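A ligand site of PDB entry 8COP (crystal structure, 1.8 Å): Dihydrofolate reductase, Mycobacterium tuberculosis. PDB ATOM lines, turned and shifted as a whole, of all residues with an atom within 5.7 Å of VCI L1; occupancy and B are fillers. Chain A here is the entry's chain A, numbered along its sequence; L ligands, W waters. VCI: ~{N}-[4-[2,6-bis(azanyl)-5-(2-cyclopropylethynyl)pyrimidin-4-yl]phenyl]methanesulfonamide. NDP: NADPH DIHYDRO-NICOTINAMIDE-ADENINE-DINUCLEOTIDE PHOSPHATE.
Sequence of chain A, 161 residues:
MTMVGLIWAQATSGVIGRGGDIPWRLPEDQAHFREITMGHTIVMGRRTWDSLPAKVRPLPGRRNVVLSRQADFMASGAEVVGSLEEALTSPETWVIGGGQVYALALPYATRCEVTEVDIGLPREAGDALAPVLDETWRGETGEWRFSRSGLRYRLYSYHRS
The backbone NH of Ala 9 lies close to a nitrogen (N04) of VCI L1, 3.5 Å away. Merely in contact with VCI L1: Ile 22, Arg 25, Gln 30, Phe 33, Thr 48, Leu 52, Tyr 102 and Thr 115. Hydrophobic or aromatic side chains that line VCI L1: Ile 7, Ala 9, Ile 22, Phe 33, Leu 52 and Ile 96. Within 4 Å of VCI L1: Ile 7, Trp 8, Ala 9, Ile 22, Arg 25, Asp 29, Gln 30, Phe 33, Thr 48, Leu 52, Ile 96, Tyr 102 and Thr 115. The nearest printed residue that does not touch VCI L1 is Leu 59 (4.7 Å).
The side-chain carboxylate of Asp 29 is in hydrogen-bond range of a nitrogen (N02) of VCI L1 (2.8 Å). O of Ile 96 is in hydrogen-bond range of N03 of VCI L1 (2.9 Å). The backbone carbonyl oxygen of Ile 7 lies within hydrogen-bond range of a nitrogen (N03) of VCI L1. A nitrogen (N04) of VCI L1 lies close to the backbone carbonyl oxygen (O) of Trp 8, 3.3 Å away. The backbone NH (N) of Thr 48 sits at hydrogen-bond distance from an oxygen (O2A) of NDP L2, at 3.3 Å. The side-chain hydroxyl (OG1) of Thr 48 sits at hydrogen-bond distance from an oxygen (O2A) of NDP L2 (2.6 Å).
OG1 of Thr 115 is in hydrogen-bond range of OD1 of Asp 29 (2.8 Å). The side-chain hydroxyl (OH) of Tyr 102 sits at hydrogen-bond distance from the backbone carbonyl oxygen (O) of Ile 96 (3.4 Å). O of Ile 7 lies within hydrogen-bond range of OH of Tyr 102. The backbone carbonyl oxygen (O) of Val 95 is in hydrogen-bond range of the backbone NH (N) of Ile 7 (3.3 Å). The backbone carbonyl oxygen of Trp 8 lies within hydrogen-bond range of the backbone NH of Thr 115. The backbone NH (N) of Trp 8 is in hydrogen-bond range of the backbone carbonyl oxygen (O) of Glu 113 (3.1 Å). The side-chain hydroxyl (OG) of Ser 51 is in hydrogen-bond range of the backbone carbonyl oxygen (O) of Thr 48, 2.9 Å away.
Water W1 lies within hydrogen-bond range of O of Glu 113, OG1 of Thr 115, N04 of VCI L1 and O of Trp 8. Water W2 lies within hydrogen-bond range of the side-chain hydroxyl (OG) of Ser 51 (3.3 Å) and an oxygen (O2D) of NDP L2 (3.4 Å).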
ATOM      1  N   ILE A   7      15.836   9.084  22.399  1.00  0.00           N
ATOM      2  CA  ILE A   7      16.244   9.258  21.025  1.00  0.00           C
ATOM      3  C   ILE A   7      15.925  10.695  20.660  1.00  0.00           C
ATOM      4  O   ILE A   7      14.828  11.173  20.943  1.00  0.00           O
ATOM      5  CB  ILE A   7      15.558   8.238  20.105  1.00  0.00           C
ATOM      6  CG1 ILE A   7      16.082   8.317  18.662  1.00  0.00           C
ATOM      7  CG2 ILE A   7      14.044   8.293  20.243  1.00  0.00           C
ATOM      8  CD1 ILE A   7      15.413   7.338  17.773  1.00  0.00           C
ATOM      9  N   TRP A   8      16.914  11.402  20.115  1.00  0.00           N
ATOM     10  CA  TRP A   8      16.669  12.754  19.632  1.00  0.00           C
ATOM     11  C   TRP A   8      17.592  13.028  18.473  1.00  0.00           C
ATOM     12  O   TRP A   8      18.578  12.324  18.249  1.00  0.00           O
ATOM     13  CB  TRP A   8      16.896  13.845  20.699  1.00  0.00           C
ATOM     14  CG  TRP A   8      18.312  14.034  21.236  1.00  0.00           C
ATOM     15  CD1 TRP A   8      19.300  14.751  20.653  1.00  0.00           C
ATOM     16  CD2 TRP A   8      18.856  13.526  22.462  1.00  0.00           C
ATOM     17  NE1 TRP A   8      20.438  14.721  21.423  1.00  0.00           N
ATOM     18  CE2 TRP A   8      20.191  13.973  22.541  1.00  0.00           C
ATOM     19  CE3 TRP A   8      18.355  12.729  23.493  1.00  0.00           C
ATOM     20  CZ2 TRP A   8      21.017  13.659  23.589  1.00  0.00           C
ATOM     21  CZ3 TRP A   8      19.178  12.426  24.534  1.00  0.00           C
ATOM     22  CH2 TRP A   8      20.503  12.881  24.574  1.00  0.00           C
ATOM     23  N   ALA A   9      17.263  14.082  17.742  1.00  0.00           N
ATOM     24  CA  ALA A   9      18.133  14.667  16.736  1.00  0.00           C
ATOM     25  C   ALA A   9      18.470  16.065  17.196  1.00  0.00           C
ATOM     26  O   ALA A   9      17.589  16.801  17.631  1.00  0.00           O
ATOM     27  CB  ALA A   9      17.452  14.733  15.372  1.00  0.00           C
ATOM     28  N   ILE A  22      10.644  21.950  14.652  1.00  0.00           N
ATOM     29  CA  ILE A  22      12.041  21.545  14.418  1.00  0.00           C
ATOM     30  C   ILE A  22      12.559  22.156  13.131  1.00  0.00           C
ATOM     31  O   ILE A  22      11.901  22.034  12.090  1.00  0.00           O
ATOM     32  CB  ILE A  22      12.176  20.025  14.344  1.00  0.00           C
ATOM     33  CG1 ILE A  22      11.701  19.374  15.630  1.00  0.00           C
ATOM     34  CG2 ILE A  22      13.626  19.642  14.176  1.00  0.00           C
ATOM     35  CD1 ILE A  22      11.294  17.930  15.419  1.00  0.00           C
ATOM     36  N   ARG A  25      14.464  18.685   8.460  1.00  0.00           N
ATOM     37  CA  ARG A  25      13.757  17.435   8.175  1.00  0.00           C
ATOM     38  C   ARG A  25      14.687  16.566   7.363  1.00  0.00           C
ATOM     39  O   ARG A  25      14.993  16.898   6.208  1.00  0.00           O
ATOM     40  CB  ARG A  25      12.436  17.673   7.454  1.00  0.00           C
ATOM     41  CG  ARG A  25      11.659  16.400   7.248  1.00  0.00           C
ATOM     42  CD  ARG A  25      10.164  16.599   7.154  1.00  0.00           C
ATOM     43  NE  ARG A  25       9.634  17.504   8.157  1.00  0.00           N
ATOM     44  CZ  ARG A  25       8.339  17.806   8.248  1.00  0.00           C
ATOM     45  NH1 ARG A  25       7.490  17.299   7.362  1.00  0.00           N
ATOM     46  NH2 ARG A  25       7.892  18.623   9.195  1.00  0.00           N
ATOM     47  N   LEU A  26      15.169  15.474   7.976  1.00  0.00           N
ATOM     48  CA  LEU A  26      16.005  14.483   7.302  1.00  0.00           C
ATOM     49  C   LEU A  26      15.233  13.179   7.221  1.00  0.00           C
ATOM     50  O   LEU A  26      14.924  12.571   8.264  1.00  0.00           O
ATOM     51  CB  LEU A  26      17.322  14.287   8.064  1.00  0.00           C
ATOM     52  CG  LEU A  26      18.423  15.320   7.857  1.00  0.00           C
ATOM     53  CD1 LEU A  26      18.124  16.678   8.504  1.00  0.00           C
ATOM     54  CD2 LEU A  26      19.726  14.766   8.394  1.00  0.00           C
ATOM     55  N   PRO A  27      14.856  12.717   6.011  1.00  0.00           N
ATOM     56  CA  PRO A  27      14.115  11.452   5.898  1.00  0.00           C
ATOM     57  C   PRO A  27      14.952  10.234   6.281  1.00  0.00           C
ATOM     58  O   PRO A  27      14.399   9.197   6.685  1.00  0.00           O
ATOM     59  CB  PRO A  27      13.714  11.413   4.415  1.00  0.00           C
ATOM     60  CG  PRO A  27      14.026  12.805   3.852  1.00  0.00           C
ATOM     61  CD  PRO A  27      15.118  13.346   4.707  1.00  0.00           C
ATOM     62  N   ASP A  29      16.644  10.335   8.945  1.00  0.00           N
ATOM     63  CA  ASP A  29      16.448  10.276  10.393  1.00  0.00           C
ATOM     64  C   ASP A  29      15.054   9.846  10.784  1.00  0.00           C
ATOM     65  O   ASP A  29      14.889   9.155  11.791  1.00  0.00           O
ATOM     66  CB  ASP A  29      16.740  11.626  11.017  1.00  0.00           C
ATOM     67  CG  ASP A  29      16.384  11.648  12.450  1.00  0.00           C
ATOM     68  OD1 ASP A  29      17.036  10.927  13.224  1.00  0.00           O
ATOM     69  OD2 ASP A  29      15.408  12.331  12.803  1.00  0.00           O
ATOM     70  N   GLN A  30      14.037  10.290  10.034  1.00  0.00           N
ATOM     71  CA  GLN A  30      12.717   9.677  10.067  1.00  0.00           C
ATOM     72  C   GLN A  30      12.805   8.153  10.108  1.00  0.00           C
ATOM     73  O   GLN A  30      12.176   7.497  10.942  1.00  0.00           O
ATOM     74  CB  GLN A  30      11.936  10.143   8.829  1.00  0.00           C
ATOM     75  CG  GLN A  30      10.595   9.440   8.560  1.00  0.00           C
ATOM     76  CD  GLN A  30       9.939   9.853   7.232  1.00  0.00           C
ATOM     77  OE1 GLN A  30      10.606   9.987   6.201  1.00  0.00           O
ATOM     78  NE2 GLN A  30       8.626  10.055   7.266  1.00  0.00           N
ATOM     79  N   HIS A  32      15.558   6.062  10.615  1.00  0.00           N
ATOM     80  CA  HIS A  32      16.243   5.576  11.810  1.00  0.00           C
ATOM     81  C   HIS A  32      15.345   5.683  13.035  1.00  0.00           C
ATOM     82  O   HIS A  32      15.204   4.718  13.794  1.00  0.00           O
ATOM     83  CB  HIS A  32      17.546   6.346  11.983  1.00  0.00           C
ATOM     84  CG  HIS A  32      18.306   6.013  13.225  1.00  0.00           C
ATOM     85  ND1 HIS A  32      18.249   6.798  14.357  1.00  0.00           N
ATOM     86  CD2 HIS A  32      19.113   4.969  13.529  1.00  0.00           C
ATOM     87  CE1 HIS A  32      19.013   6.264  15.300  1.00  0.00           C
ATOM     88  NE2 HIS A  32      19.551   5.157  14.822  1.00  0.00           N
ATOM     89  N   PHE A  33      14.666   6.821  13.184  1.00  0.00           N
ATOM     90  CA  PHE A  33      13.842   6.998  14.362  1.00  0.00           C
ATOM     91  C   PHE A  33      12.711   5.989  14.359  1.00  0.00           C
ATOM     92  O   PHE A  33      12.352   5.442  15.399  1.00  0.00           O
ATOM     93  CB  PHE A  33      13.298   8.420  14.425  1.00  0.00           C
ATOM     94  CG  PHE A  33      12.023   8.556  15.205  1.00  0.00           C
ATOM     95  CD1 PHE A  33      12.057   8.446  16.591  1.00  0.00           C
ATOM     96  CD2 PHE A  33      10.816   8.748  14.593  1.00  0.00           C
ATOM     97  CE1 PHE A  33      10.924   8.568  17.352  1.00  0.00           C
ATOM     98  CE2 PHE A  33       9.667   8.855  15.351  1.00  0.00           C
ATOM     99  CZ  PHE A  33       9.726   8.766  16.731  1.00  0.00           C
ATOM    100  N   THR A  48       4.949  18.282  22.727  1.00  0.00           N
ATOM    101  CA  THR A  48       5.305  17.526  21.520  1.00  0.00           C
ATOM    102  C   THR A  48       4.099  16.855  20.852  1.00  0.00           C
ATOM    103  O   THR A  48       4.010  16.817  19.627  1.00  0.00           O
ATOM    104  CB  THR A  48       6.366  16.465  21.873  1.00  0.00           C
ATOM    105  OG1 THR A  48       7.607  17.116  22.173  1.00  0.00           O
ATOM    106  CG2 THR A  48       6.574  15.473  20.724  1.00  0.00           C
ATOM    107  N   SER A  51       2.295  19.423  18.379  1.00  0.00           N
ATOM    108  CA  SER A  51       2.949  19.827  17.138  1.00  0.00           C
ATOM    109  C   SER A  51       2.588  18.904  16.006  1.00  0.00           C
ATOM    110  O   SER A  51       2.421  19.339  14.863  1.00  0.00           O
ATOM    111  CB  SER A  51       4.462  19.861  17.313  1.00  0.00           C
ATOM    112  OG  SER A  51       4.972  18.541  17.515  1.00  0.00           O
ATOM    113  N   LEU A  52       2.435  17.642  16.318  1.00  0.00           N
ATOM    114  CA  LEU A  52       2.026  16.528  15.479  1.00  0.00           C
ATOM    115  C   LEU A  52       0.631  16.748  14.901  1.00  0.00           C
ATOM    116  O   LEU A  52      -0.348  16.778  15.665  1.00  0.00           O
ATOM    117  CB  LEU A  52       2.023  15.278  16.336  1.00  0.00           C
ATOM    118  CG  LEU A  52       3.382  14.943  16.896  1.00  0.00           C
ATOM    119  CD1 LEU A  52       3.260  13.759  17.806  1.00  0.00           C
ATOM    120  CD2 LEU A  52       4.345  14.683  15.754  1.00  0.00           C
ATOM    121  N   LEU A  59       1.458   7.809  16.427  1.00  0.00           N
ATOM    122  CA  LEU A  59       2.433   7.096  15.613  1.00  0.00           C
ATOM    123  C   LEU A  59       2.079   5.618  15.597  1.00  0.00           C
ATOM    124  O   LEU A  59       1.905   5.012  16.677  1.00  0.00           O
ATOM    125  CB  LEU A  59       3.834   7.293  16.183  1.00  0.00           C
ATOM    126  CG  LEU A  59       4.568   8.605  15.905  1.00  0.00           C
ATOM    127  CD1 LEU A  59       3.953   9.751  16.674  1.00  0.00           C
ATOM    128  CD2 LEU A  59       6.021   8.468  16.285  1.00  0.00           C
ATOM    129  N   VAL A  95      11.658   7.653  25.128  1.00  0.00           N
ATOM    130  CA  VAL A  95      11.375   9.064  25.313  1.00  0.00           C
ATOM    131  C   VAL A  95      11.709   9.761  24.003  1.00  0.00           C
ATOM    132  O   VAL A  95      12.876   9.812  23.615  1.00  0.00           O
ATOM    133  CB  VAL A  95      12.192   9.631  26.463  1.00  0.00           C
ATOM    134  CG1 VAL A  95      11.802  11.066  26.751  1.00  0.00           C
ATOM    135  CG2 VAL A  95      12.037   8.743  27.687  1.00  0.00           C
ATOM    136  N   ILE A  96      10.702  10.297  23.328  1.00  0.00           N
ATOM    137  CA  ILE A  96      10.927  10.848  21.984  1.00  0.00           C
ATOM    138  C   ILE A  96      10.807  12.369  21.954  1.00  0.00           C
ATOM    139  O   ILE A  96      10.833  12.948  20.873  1.00  0.00           O
ATOM    140  CB  ILE A  96       9.993  10.198  20.962  1.00  0.00           C
ATOM    141  CG1 ILE A  96       8.529  10.499  21.295  1.00  0.00           C
ATOM    142  CG2 ILE A  96      10.223   8.691  20.992  1.00  0.00           C
ATOM    143  CD1 ILE A  96       7.594  10.095  20.201  1.00  0.00           C
ATOM    144  N   GLY A  97      10.695  13.026  23.097  1.00  0.00           N
ATOM    145  CA  GLY A  97      10.787  14.463  23.152  1.00  0.00           C
ATOM    146  C   GLY A  97       9.722  15.083  24.039  1.00  0.00           C
ATOM    147  O   GLY A  97       8.784  14.426  24.501  1.00  0.00           O
ATOM    148  N   TYR A 102      13.049  15.212  28.110  1.00  0.00           N
ATOM    149  CA  TYR A 102      14.371  14.621  28.038  1.00  0.00           C
ATOM    150  C   TYR A 102      15.066  14.681  29.393  1.00  0.00           C
ATOM    151  O   TYR A 102      15.449  13.650  29.942  1.00  0.00           O
ATOM    152  CB  TYR A 102      15.244  15.306  26.985  1.00  0.00           C
ATOM    153  CG  TYR A 102      14.943  14.869  25.572  1.00  0.00           C
ATOM    154  CD1 TYR A 102      14.997  15.785  24.524  1.00  0.00           C
ATOM    155  CD2 TYR A 102      14.556  13.569  25.294  1.00  0.00           C
ATOM    156  CE1 TYR A 102      14.683  15.407  23.240  1.00  0.00           C
ATOM    157  CE2 TYR A 102      14.254  13.182  24.017  1.00  0.00           C
ATOM    158  CZ  TYR A 102      14.325  14.109  22.992  1.00  0.00           C
ATOM    159  OH  TYR A 102      14.008  13.772  21.709  1.00  0.00           O
ATOM    160  N   GLU A 113      19.983   7.507  21.709  1.00  0.00           N
ATOM    161  CA  GLU A 113      20.257   7.383  20.274  1.00  0.00           C
ATOM    162  C   GLU A 113      20.170   8.756  19.616  1.00  0.00           C
ATOM    163  O   GLU A 113      19.073   9.249  19.356  1.00  0.00           O
ATOM    164  CB  GLU A 113      19.295   6.402  19.601  1.00  0.00           C
ATOM    165  CG  GLU A 113      19.485   4.968  20.002  1.00  0.00           C
ATOM    166  CD  GLU A 113      20.761   4.367  19.423  1.00  0.00           C
ATOM    167  OE1 GLU A 113      21.130   4.698  18.266  1.00  0.00           O
ATOM    168  OE2 GLU A 113      21.391   3.558  20.134  1.00  0.00           O
ATOM    169  N   VAL A 114      21.303   9.340  19.303  1.00  0.00           N
ATOM    170  CA  VAL A 114      21.394  10.743  18.916  1.00  0.00           C
ATOM    171  C   VAL A 114      21.740  10.827  17.438  1.00  0.00           C
ATOM    172  O   VAL A 114      22.788  10.327  17.016  1.00  0.00           O
ATOM    173  CB  VAL A 114      22.449  11.470  19.758  1.00  0.00           C
ATOM    174  CG1 VAL A 114      22.482  12.949  19.423  1.00  0.00           C
ATOM    175  CG2 VAL A 114      22.149  11.240  21.227  1.00  0.00           C
ATOM    176  N   THR A 115      20.920  11.516  16.661  1.00  0.00           N
ATOM    177  CA  THR A 115      21.321  11.906  15.322  1.00  0.00           C
ATOM    178  C   THR A 115      21.882  13.315  15.406  1.00  0.00           C
ATOM    179  O   THR A 115      21.196  14.229  15.859  1.00  0.00           O
ATOM    180  CB  THR A 115      20.171  11.841  14.322  1.00  0.00           C
ATOM    181  OG1 THR A 115      19.632  10.516  14.322  1.00  0.00           O
ATOM    182  CG2 THR A 115      20.670  12.159  12.931  1.00  0.00           C
HETATM  183  C10 VCI L   1      10.549  14.687  13.406  1.00  0.00           C
HETATM  184  C11 VCI L   1      10.548  14.068  12.184  1.00  0.00           C
HETATM  185  C16 VCI L   1       7.274  13.046  16.846  1.00  0.00           C
HETATM  186  C01 VCI L   1      14.983  11.569  16.278  1.00  0.00           C
HETATM  187  C02 VCI L   1      12.848  12.411  15.430  1.00  0.00           C
HETATM  188  C03 VCI L   1      12.320  12.299  16.710  1.00  0.00           C
HETATM  189  C04 VCI L   1      13.186  11.807  17.660  1.00  0.00           C
HETATM  190  C05 VCI L   1      10.888  12.658  17.109  1.00  0.00           C
HETATM  191  C06 VCI L   1       9.775  12.912  17.439  1.00  0.00           C
HETATM  192  C07 VCI L   1      12.028  12.959  14.245  1.00  0.00           C
HETATM  193  C08 VCI L   1       8.361  13.272  17.900  1.00  0.00           C
HETATM  194  C09 VCI L   1      11.291  14.143  14.439  1.00  0.00           C
HETATM  195  C12 VCI L   1      11.268  12.910  11.956  1.00  0.00           C
HETATM  196  C13 VCI L   1      12.016  12.348  12.984  1.00  0.00           C
HETATM  197  C14 VCI L   1       7.633  14.540   9.171  1.00  0.00           C
HETATM  198  C15 VCI L   1       7.749  14.460  17.171  1.00  0.00           C
HETATM  199  N01 VCI L   1      14.447  11.456  17.507  1.00  0.00           N
HETATM  200  N02 VCI L   1      14.152  12.049  15.334  1.00  0.00           N
HETATM  201  N03 VCI L   1      12.629  11.680  19.000  1.00  0.00           N
HETATM  202  N04 VCI L   1      16.372  11.195  16.001  1.00  0.00           N
HETATM  203  N05 VCI L   1       9.764  14.681  11.128  1.00  0.00           N
HETATM  204  O01 VCI L   1       8.694  12.408  10.448  1.00  0.00           O
HETATM  205  O02 VCI L   1      10.108  13.382   8.894  1.00  0.00           O
HETATM  206  S01 VCI L   1       9.096  13.718   9.892  1.00  0.00           S
HETATM  207  PA  NDP L   2       7.890  18.985  25.802  1.00  0.00           P
HETATM  208  O1A NDP L   2       8.953  18.598  26.761  1.00  0.00           O
HETATM  209  O2A NDP L   2       7.792  18.395  24.436  1.00  0.00           O
HETATM  210  O5B NDP L   2       6.432  18.783  26.482  1.00  0.00           O
HETATM  211  C5B NDP L   2       6.425  19.610  27.602  1.00  0.00           C
HETATM  212  C4B NDP L   2       5.210  19.218  28.400  1.00  0.00           C
HETATM  213  O4B NDP L   2       5.526  18.124  29.225  1.00  0.00           O
HETATM  214  C3B NDP L   2       4.781  20.345  29.344  1.00  0.00           C
HETATM  215  O3B NDP L   2       4.047  21.287  28.618  1.00  0.00           O
HETATM  216  C2B NDP L   2       3.838  19.567  30.292  1.00  0.00           C
HETATM  217  O2B NDP L   2       2.659  19.326  29.754  1.00  0.00           O
HETATM  218  C1B NDP L   2       4.575  18.154  30.308  1.00  0.00           C
HETATM  219  N9A NDP L   2       5.285  17.848  31.548  1.00  0.00           N
HETATM  220  C8A NDP L   2       6.561  18.237  31.935  1.00  0.00           C
HETATM  221  N7A NDP L   2       6.917  17.760  33.143  1.00  0.00           N
HETATM  222  C5A NDP L   2       5.807  17.025  33.561  1.00  0.00           C
HETATM  223  C6A NDP L   2       5.552  16.297  34.716  1.00  0.00           C
HETATM  224  N6A NDP L   2       6.504  16.224  35.708  1.00  0.00           N
HETATM  225  N1A NDP L   2       4.392  15.650  34.910  1.00  0.00           N
HETATM  226  C2A NDP L   2       3.480  15.764  33.896  1.00  0.00           C
HETATM  227  N3A NDP L   2       3.582  16.414  32.727  1.00  0.00           N
HETATM  228  C4A NDP L   2       4.791  17.063  32.583  1.00  0.00           C
HETATM  229  O3  NDP L   2       8.059  20.602  25.683  1.00  0.00           O
HETATM  230  PN  NDP L   2       9.402  21.103  25.001  1.00  0.00           P
HETATM  231  O1N NDP L   2      10.527  20.959  25.938  1.00  0.00           O
HETATM  232  O2N NDP L   2       9.181  22.414  24.291  1.00  0.00           O
HETATM  233  O5D NDP L   2       9.866  20.087  23.683  1.00  0.00           O
HETATM  234  C5D NDP L   2       9.137  20.503  22.574  1.00  0.00           C
HETATM  235  C4D NDP L   2      10.113  20.898  21.475  1.00  0.00           C
HETATM  236  O4D NDP L   2      11.012  19.812  21.198  1.00  0.00           O
HETATM  237  C3D NDP L   2       9.321  21.206  20.166  1.00  0.00           C
HETATM  238  O3D NDP L   2       9.985  22.254  19.575  1.00  0.00           O
HETATM  239  C2D NDP L   2       9.536  19.976  19.348  1.00  0.00           C
HETATM  240  O2D NDP L   2       9.556  20.280  17.990  1.00  0.00           O
HETATM  241  C1D NDP L   2      11.002  19.613  19.815  1.00  0.00           C
HETATM  242  N1N NDP L   2      11.311  18.171  19.538  1.00  0.00           N
HETATM  243  C2N NDP L   2      12.512  17.808  18.950  1.00  0.00           C
HETATM  244  C3N NDP L   2      12.856  16.491  18.860  1.00  0.00           C
HETATM  245  C7N NDP L   2      14.128  16.178  18.210  1.00  0.00           C
HETATM  246  O7N NDP L   2      14.821  17.004  17.592  1.00  0.00           O
HETATM  247  N7N NDP L   2      14.584  14.880  18.306  1.00  0.00           N
HETATM  248  C4N NDP L   2      11.994  15.417  19.389  1.00  0.00           C
HETATM  249  C5N NDP L   2      10.680  15.897  19.804  1.00  0.00           C
HETATM  250  C6N NDP L   2      10.385  17.192  19.877  1.00  0.00           C
HETATM  251  P2B NDP L   2       1.243  20.356  30.221  1.00  0.00           P
HETATM  252  O1X NDP L   2       1.700  21.608  29.545  1.00  0.00           O
HETATM  253  O2X NDP L   2       0.011  19.654  29.639  1.00  0.00           O
HETATM  254  O3X NDP L   2       1.438  20.254  31.696  1.00  0.00           O
HETATM  255  O   HOH W   1      18.642   9.605  16.725  1.00  0.00           O
HETATM  256  O   HOH W   2       8.039  17.540  16.762  1.00  0.00           O
